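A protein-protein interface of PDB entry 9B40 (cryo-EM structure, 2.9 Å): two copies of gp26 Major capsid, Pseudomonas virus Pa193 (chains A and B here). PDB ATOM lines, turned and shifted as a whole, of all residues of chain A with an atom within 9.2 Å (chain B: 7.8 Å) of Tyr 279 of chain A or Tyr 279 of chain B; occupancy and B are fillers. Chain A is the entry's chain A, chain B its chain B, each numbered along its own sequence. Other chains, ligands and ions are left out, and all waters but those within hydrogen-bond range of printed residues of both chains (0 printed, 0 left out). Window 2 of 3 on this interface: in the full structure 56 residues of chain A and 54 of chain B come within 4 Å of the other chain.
NE2 of Gln 289 of chain A lies within hydrogen-bond range of OG of Ser 282 of chain B (2.7 Å).
The indole nitrogen (NE1) of Trp 232 of chain A sits at hydrogen-bond distance from the backbone carbonyl oxygen (O) of Ile 281 of chain A (3.1 Å). NE1 of Trp 232 of chain A sits at hydrogen-bond distance from O of Ser 282 of chain A, 3.5 Å away. OD1 of Asp 285 of chain A sits close to OE1 of Gln 289 of chain A (3.3 Å).
Among the printed residues, pairs that only touch across the chains: Trp 232 of chain A with Thr 276 of chain B (3.6 Å), Trp 232 of chain A with Gly 280 of chain B (3.5 Å), Thr 277 of chain A with Pro 278 of chain B (3.7 Å), Thr 277 of chain A with Tyr 279 of chain B (3.8 Å), Tyr 279 of chain A with Tyr 279 of chain B (3.3 Å), Ile 281 of chain A with Tyr 279 of chain B (3.5 Å), Ile 281 of chain A with Gly 280 of chain B (3.3 Å), Trp 286 of chain A with Thr 276 of chain B (3.3 Å), Trp 286 of chain A with Ser 282 of chain B (3.3 Å), Gln 289 of chain A with Gly 280 of chain B (3.6 Å) and Gln 289 of chain A with Ile 281 of chain B (3.7 Å).
Tyr 279 of chain A touches one residue of chain B. Tyr 279 of chain B touches just these residues of chain A: Thr 277 (3.8 Å), Tyr 279 (3.3 Å) and Ile 281 (3.5 Å). No residue of chain A comes within 4 Å of Thr 277 of chain B. Of chain A, only Thr 277 (3.7 Å) comes within 4 Å of Pro 278 of chain B. Of chain A, only Trp 232, Ile 281 and Gln 289 come within 4 Å of Gly 280 of chain B. Of the printed residues of chain B, Ile 281 of chain A touches Tyr 279 and Gly 280. Printed residues of chain A within 4 Å of Thr 276 of chain B: Trp 232 and Trp 286. Of the printed residues of chain B, Gln 289 of chain A touches Gly 280 (3.6 Å), Ile 281 (3.7 Å) and Ser 282 (2.7 Å). Ile 236 of chain A touches none of the printed residues of chain B. Val 275 of chain A touches none of the printed residues of chain B. The nearest residue of chain B that does not touch Tyr 279 of chain A is Pro 278 of chain B (4.8 Å). The nearest residue of chain A that does not touch Tyr 279 of chain B is Trp 232 of chain A (5.1 Å). The nearest printed residue of chain B that does not touch Trp 286 of chain A is Gly 280 of chain B (6.0 Å).
Hydrophobic or aromatic side chains of chain A that line the printed part of chain B: Trp 232, Tyr 279, Ile 281 and Trp 286. Printed residues of chain B that touch a printed residue of chain A: Thr 276, Pro 278, Tyr 279, Gly 280, Ile 281 and Ser 282. Among the printed residues, 12 pairs touch across the chains.
Thr 277 of chain A touches Pro 278 of chain B, but with the chains exchanged Pro 278 of chain A does not touch Thr 277 of chain B (9.7 Å). Thr 277 of chain A touches Tyr 279 of chain B, but with the chains exchanged Tyr 279 of chain A does not touch Thr 277 of chain B (8.2 Å). Tyr 279 of chain A touches its own counterpart, Tyr 279 of chain B. Ile 281 of chain A touches Gly 280 of chain B, but with the chains exchanged Gly 280 of chain A does not touch Ile 281 of chain B (7.8 Å). 7 positions are printed for both chains. Of the 12 pairs that touch across the chains among the printed residues, 1 has its exchanged pair printed and touching as well.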
ATOM      1  N   TRP A 232      14.105 -24.858  11.628  1.00  0.00           N
ATOM      2  CA  TRP A 232      14.691 -23.735  12.354  1.00  0.00           C
ATOM      3  C   TRP A 232      13.634 -22.698  12.719  1.00  0.00           C
ATOM      4  O   TRP A 232      13.624 -22.175  13.843  1.00  0.00           O
ATOM      5  CB  TRP A 232      15.801 -23.114  11.505  1.00  0.00           C
ATOM      6  CG  TRP A 232      16.416 -21.882  12.069  1.00  0.00           C
ATOM      7  CD1 TRP A 232      17.471 -21.813  12.928  1.00  0.00           C
ATOM      8  CD2 TRP A 232      16.039 -20.531  11.788  1.00  0.00           C
ATOM      9  NE1 TRP A 232      17.765 -20.503  13.212  1.00  0.00           N
ATOM     10  CE2 TRP A 232      16.900 -19.696  12.522  1.00  0.00           C
ATOM     11  CE3 TRP A 232      15.048 -19.947  10.993  1.00  0.00           C
ATOM     12  CZ2 TRP A 232      16.802 -18.310  12.487  1.00  0.00           C
ATOM     13  CZ3 TRP A 232      14.953 -18.572  10.959  1.00  0.00           C
ATOM     14  CH2 TRP A 232      15.823 -17.768  11.703  1.00  0.00           C
ATOM     15  N   ALA A 233      12.727 -22.405  11.783  1.00  0.00           N
ATOM     16  CA  ALA A 233      11.697 -21.397  12.015  1.00  0.00           C
ATOM     17  C   ALA A 233      10.767 -21.794  13.153  1.00  0.00           C
ATOM     18  O   ALA A 233      10.320 -20.937  13.920  1.00  0.00           O
ATOM     19  CB  ALA A 233      10.901 -21.157  10.733  1.00  0.00           C
ATOM     20  N   ILE A 236      12.622 -21.190  16.458  1.00  0.00           N
ATOM     21  CA  ILE A 236      12.661 -19.743  16.662  1.00  0.00           C
ATOM     22  C   ILE A 236      11.301 -19.228  17.113  1.00  0.00           C
ATOM     23  O   ILE A 236      11.210 -18.396  18.023  1.00  0.00           O
ATOM     24  CB  ILE A 236      13.144 -19.037  15.381  1.00  0.00           C
ATOM     25  CG1 ILE A 236      14.606 -19.368  15.067  1.00  0.00           C
ATOM     26  CG2 ILE A 236      12.955 -17.537  15.475  1.00  0.00           C
ATOM     27  CD1 ILE A 236      15.480 -19.709  16.262  1.00  0.00           C
ATOM     28  N   VAL A 275      20.440 -26.588  15.450  1.00  0.00           N
ATOM     29  CA  VAL A 275      19.748 -26.771  14.180  1.00  0.00           C
ATOM     30  C   VAL A 275      19.745 -25.461  13.409  1.00  0.00           C
ATOM     31  O   VAL A 275      19.439 -24.393  13.955  1.00  0.00           O
ATOM     32  CB  VAL A 275      18.321 -27.293  14.425  1.00  0.00           C
ATOM     33  CG1 VAL A 275      17.433 -27.058  13.213  1.00  0.00           C
ATOM     34  CG2 VAL A 275      18.358 -28.767  14.788  1.00  0.00           C
ATOM     35  N   THR A 276      20.089 -25.539  12.128  1.00  0.00           N
ATOM     36  CA  THR A 276      20.277 -24.363  11.298  1.00  0.00           C
ATOM     37  C   THR A 276      19.202 -24.274  10.228  1.00  0.00           C
ATOM     38  O   THR A 276      18.639 -25.283   9.793  1.00  0.00           O
ATOM     39  CB  THR A 276      21.642 -24.376  10.605  1.00  0.00           C
ATOM     40  OG1 THR A 276      21.756 -25.552   9.794  1.00  0.00           O
ATOM     41  CG2 THR A 276      22.749 -24.372  11.622  1.00  0.00           C
ATOM     42  N   THR A 277      18.932 -23.043   9.812  1.00  0.00           N
ATOM     43  CA  THR A 277      18.314 -22.815   8.522  1.00  0.00           C
ATOM     44  C   THR A 277      19.262 -23.339   7.442  1.00  0.00           C
ATOM     45  O   THR A 277      20.479 -23.387   7.653  1.00  0.00           O
ATOM     46  CB  THR A 277      18.031 -21.318   8.344  1.00  0.00           C
ATOM     47  OG1 THR A 277      17.418 -21.065   7.075  1.00  0.00           O
ATOM     48  CG2 THR A 277      19.307 -20.507   8.457  1.00  0.00           C
ATOM     49  N   PRO A 278      18.744 -23.766   6.284  1.00  0.00           N
ATOM     50  CA  PRO A 278      19.635 -24.296   5.232  1.00  0.00           C
ATOM     51  C   PRO A 278      20.678 -23.310   4.710  1.00  0.00           C
ATOM     52  O   PRO A 278      21.439 -23.674   3.805  1.00  0.00           O
ATOM     53  CB  PRO A 278      18.661 -24.710   4.120  1.00  0.00           C
ATOM     54  CG  PRO A 278      17.369 -24.936   4.816  1.00  0.00           C
ATOM     55  CD  PRO A 278      17.323 -23.952   5.937  1.00  0.00           C
ATOM     56  N   TYR A 279      20.742 -22.091   5.243  1.00  0.00           N
ATOM     57  CA  TYR A 279      21.645 -21.066   4.753  1.00  0.00           C
ATOM     58  C   TYR A 279      22.711 -20.698   5.778  1.00  0.00           C
ATOM     59  O   TYR A 279      23.491 -19.772   5.536  1.00  0.00           O
ATOM     60  CB  TYR A 279      20.861 -19.813   4.327  1.00  0.00           C
ATOM     61  CG  TYR A 279      19.666 -20.075   3.411  1.00  0.00           C
ATOM     62  CD1 TYR A 279      18.504 -20.687   3.883  1.00  0.00           C
ATOM     63  CD2 TYR A 279      19.653 -19.602   2.115  1.00  0.00           C
ATOM     64  CE1 TYR A 279      17.422 -20.906   3.063  1.00  0.00           C
ATOM     65  CE2 TYR A 279      18.574 -19.827   1.278  1.00  0.00           C
ATOM     66  CZ  TYR A 279      17.456 -20.464   1.764  1.00  0.00           C
ATOM     67  OH  TYR A 279      16.371 -20.669   0.942  1.00  0.00           O
ATOM     68  N   GLY A 280      22.756 -21.392   6.914  1.00  0.00           N
ATOM     69  CA  GLY A 280      23.851 -21.276   7.858  1.00  0.00           C
ATOM     70  C   GLY A 280      23.662 -20.329   9.025  1.00  0.00           C
ATOM     71  O   GLY A 280      24.575 -19.570   9.357  1.00  0.00           O
ATOM     72  N   ILE A 281      22.500 -20.375   9.676  1.00  0.00           N
ATOM     73  CA  ILE A 281      22.237 -19.602  10.888  1.00  0.00           C
ATOM     74  C   ILE A 281      21.569 -20.541  11.883  1.00  0.00           C
ATOM     75  O   ILE A 281      20.444 -20.994  11.650  1.00  0.00           O
ATOM     76  CB  ILE A 281      21.356 -18.368  10.639  1.00  0.00           C
ATOM     77  CG1 ILE A 281      22.023 -17.399   9.658  1.00  0.00           C
ATOM     78  CG2 ILE A 281      21.039 -17.667  11.950  1.00  0.00           C
ATOM     79  CD1 ILE A 281      23.244 -16.708  10.218  1.00  0.00           C
ATOM     80  N   SER A 282      22.256 -20.838  12.980  1.00  0.00           N
ATOM     81  CA  SER A 282      21.729 -21.749  13.980  1.00  0.00           C
ATOM     82  C   SER A 282      20.775 -21.024  14.926  1.00  0.00           C
ATOM     83  O   SER A 282      20.672 -19.795  14.933  1.00  0.00           O
ATOM     84  CB  SER A 282      22.867 -22.397  14.766  1.00  0.00           C
ATOM     85  OG  SER A 282      23.595 -21.430  15.498  1.00  0.00           O
ATOM     86  N   ASP A 285      22.789 -18.908  17.244  1.00  0.00           N
ATOM     87  CA  ASP A 285      23.141 -17.619  16.657  1.00  0.00           C
ATOM     88  C   ASP A 285      21.970 -16.646  16.752  1.00  0.00           C
ATOM     89  O   ASP A 285      22.162 -15.459  17.040  1.00  0.00           O
ATOM     90  CB  ASP A 285      23.573 -17.819  15.202  1.00  0.00           C
ATOM     91  CG  ASP A 285      24.221 -16.583  14.585  1.00  0.00           C
ATOM     92  OD1 ASP A 285      24.224 -15.496  15.198  1.00  0.00           O
ATOM     93  OD2 ASP A 285      24.773 -16.713  13.473  1.00  0.00           O
ATOM     94  N   TRP A 286      20.750 -17.135  16.519  1.00  0.00           N
ATOM     95  CA  TRP A 286      19.569 -16.285  16.644  1.00  0.00           C
ATOM     96  C   TRP A 286      19.392 -15.786  18.072  1.00  0.00           C
ATOM     97  O   TRP A 286      19.077 -14.611  18.292  1.00  0.00           O
ATOM     98  CB  TRP A 286      18.325 -17.044  16.187  1.00  0.00           C
ATOM     99  CG  TRP A 286      17.065 -16.269  16.379  1.00  0.00           C
ATOM    100  CD1 TRP A 286      16.557 -15.322  15.547  1.00  0.00           C
ATOM    101  CD2 TRP A 286      16.159 -16.358  17.484  1.00  0.00           C
ATOM    102  NE1 TRP A 286      15.387 -14.820  16.057  1.00  0.00           N
ATOM    103  CE2 TRP A 286      15.121 -15.439  17.248  1.00  0.00           C
ATOM    104  CE3 TRP A 286      16.125 -17.128  18.648  1.00  0.00           C
ATOM    105  CZ2 TRP A 286      14.061 -15.270  18.131  1.00  0.00           C
ATOM    106  CZ3 TRP A 286      15.073 -16.959  19.522  1.00  0.00           C
ATOM    107  CH2 TRP A 286      14.055 -16.037  19.260  1.00  0.00           C
ATOM    108  N   GLN A 289      22.108 -13.119  18.746  1.00  0.00           N
ATOM    109  CA  GLN A 289      21.834 -11.846  18.096  1.00  0.00           C
ATOM    110  C   GLN A 289      20.508 -11.238  18.526  1.00  0.00           C
ATOM    111  O   GLN A 289      20.217 -10.098  18.151  1.00  0.00           O
ATOM    112  CB  GLN A 289      21.848 -12.008  16.572  1.00  0.00           C
ATOM    113  CG  GLN A 289      20.609 -12.668  15.997  1.00  0.00           C
ATOM    114  CD  GLN A 289      20.803 -13.114  14.562  1.00  0.00           C
ATOM    115  OE1 GLN A 289      21.923 -13.380  14.130  1.00  0.00           O
ATOM    116  NE2 GLN A 289      19.712 -13.195  13.815  1.00  0.00           N
ATOM    117  N   THR B 276      12.590 -12.334  12.074  1.00  0.00           N
ATOM    118  CA  THR B 276      13.702 -12.543  11.164  1.00  0.00           C
ATOM    119  C   THR B 276      13.224 -12.671   9.727  1.00  0.00           C
ATOM    120  O   THR B 276      12.077 -13.041   9.458  1.00  0.00           O
ATOM    121  CB  THR B 276      14.493 -13.805  11.517  1.00  0.00           C
ATOM    122  OG1 THR B 276      13.654 -14.957  11.362  1.00  0.00           O
ATOM    123  CG2 THR B 276      14.981 -13.739  12.937  1.00  0.00           C
ATOM    124  N   THR B 277      14.135 -12.360   8.811  1.00  0.00           N
ATOM    125  CA  THR B 277      14.029 -12.831   7.450  1.00  0.00           C
ATOM    126  C   THR B 277      14.095 -14.359   7.467  1.00  0.00           C
ATOM    127  O   THR B 277      14.679 -14.948   8.381  1.00  0.00           O
ATOM    128  CB  THR B 277      15.161 -12.226   6.608  1.00  0.00           C
ATOM    129  OG1 THR B 277      15.064 -12.651   5.245  1.00  0.00           O
ATOM    130  CG2 THR B 277      16.517 -12.613   7.163  1.00  0.00           C
ATOM    131  N   PRO B 278      13.482 -15.033   6.486  1.00  0.00           N
ATOM    132  CA  PRO B 278      13.524 -16.508   6.471  1.00  0.00           C
ATOM    133  C   PRO B 278      14.922 -17.115   6.374  1.00  0.00           C
ATOM    134  O   PRO B 278      15.033 -18.348   6.360  1.00  0.00           O
ATOM    135  CB  PRO B 278      12.674 -16.872   5.246  1.00  0.00           C
ATOM    136  CG  PRO B 278      11.783 -15.701   5.045  1.00  0.00           C
ATOM    137  CD  PRO B 278      12.582 -14.507   5.444  1.00  0.00           C
ATOM    138  N   TYR B 279      15.979 -16.308   6.307  1.00  0.00           N
ATOM    139  CA  TYR B 279      17.335 -16.803   6.131  1.00  0.00           C
ATOM    140  C   TYR B 279      18.184 -16.589   7.378  1.00  0.00           C
ATOM    141  O   TYR B 279      19.393 -16.845   7.348  1.00  0.00           O
ATOM    142  CB  TYR B 279      18.004 -16.158   4.908  1.00  0.00           C
ATOM    143  CG  TYR B 279      17.173 -16.126   3.624  1.00  0.00           C
ATOM    144  CD1 TYR B 279      16.008 -15.365   3.518  1.00  0.00           C
ATOM    145  CD2 TYR B 279      17.525 -16.909   2.542  1.00  0.00           C
ATOM    146  CE1 TYR B 279      15.253 -15.360   2.368  1.00  0.00           C
ATOM    147  CE2 TYR B 279      16.765 -16.919   1.386  1.00  0.00           C
ATOM    148  CZ  TYR B 279      15.637 -16.135   1.304  1.00  0.00           C
ATOM    149  OH  TYR B 279      14.885 -16.135   0.152  1.00  0.00           O
ATOM    150  N   GLY B 280      17.578 -16.127   8.470  1.00  0.00           N
ATOM    151  CA  GLY B 280      18.232 -16.061   9.763  1.00  0.00           C
ATOM    152  C   GLY B 280      18.953 -14.772  10.102  1.00  0.00           C
ATOM    153  O   GLY B 280      20.094 -14.807  10.568  1.00  0.00           O
ATOM    154  N   ILE B 281      18.299 -13.630   9.896  1.00  0.00           N
ATOM    155  CA  ILE B 281      18.815 -12.336  10.334  1.00  0.00           C
ATOM    156  C   ILE B 281      17.676 -11.591  11.013  1.00  0.00           C
ATOM    157  O   ILE B 281      16.636 -11.347  10.391  1.00  0.00           O
ATOM    158  CB  ILE B 281      19.385 -11.494   9.178  1.00  0.00           C
ATOM    159  CG1 ILE B 281      20.551 -12.210   8.492  1.00  0.00           C
ATOM    160  CG2 ILE B 281      19.817 -10.127   9.680  1.00  0.00           C
ATOM    161  CD1 ILE B 281      21.798 -12.301   9.343  1.00  0.00           C
ATOM    162  N   SER B 282      17.868 -11.225  12.273  1.00  0.00           N
ATOM    163  CA  SER B 282      16.832 -10.560  13.046  1.00  0.00           C
ATOM    164  C   SER B 282      16.865  -9.055  12.821  1.00  0.00           C
ATOM    165  O   SER B 282      17.834  -8.497  12.303  1.00  0.00           O
ATOM    166  CB  SER B 282      16.988 -10.864  14.536  1.00  0.00           C
ATOM    167  OG  SER B 282      17.418 -12.197  14.743  1.00  0.00           O
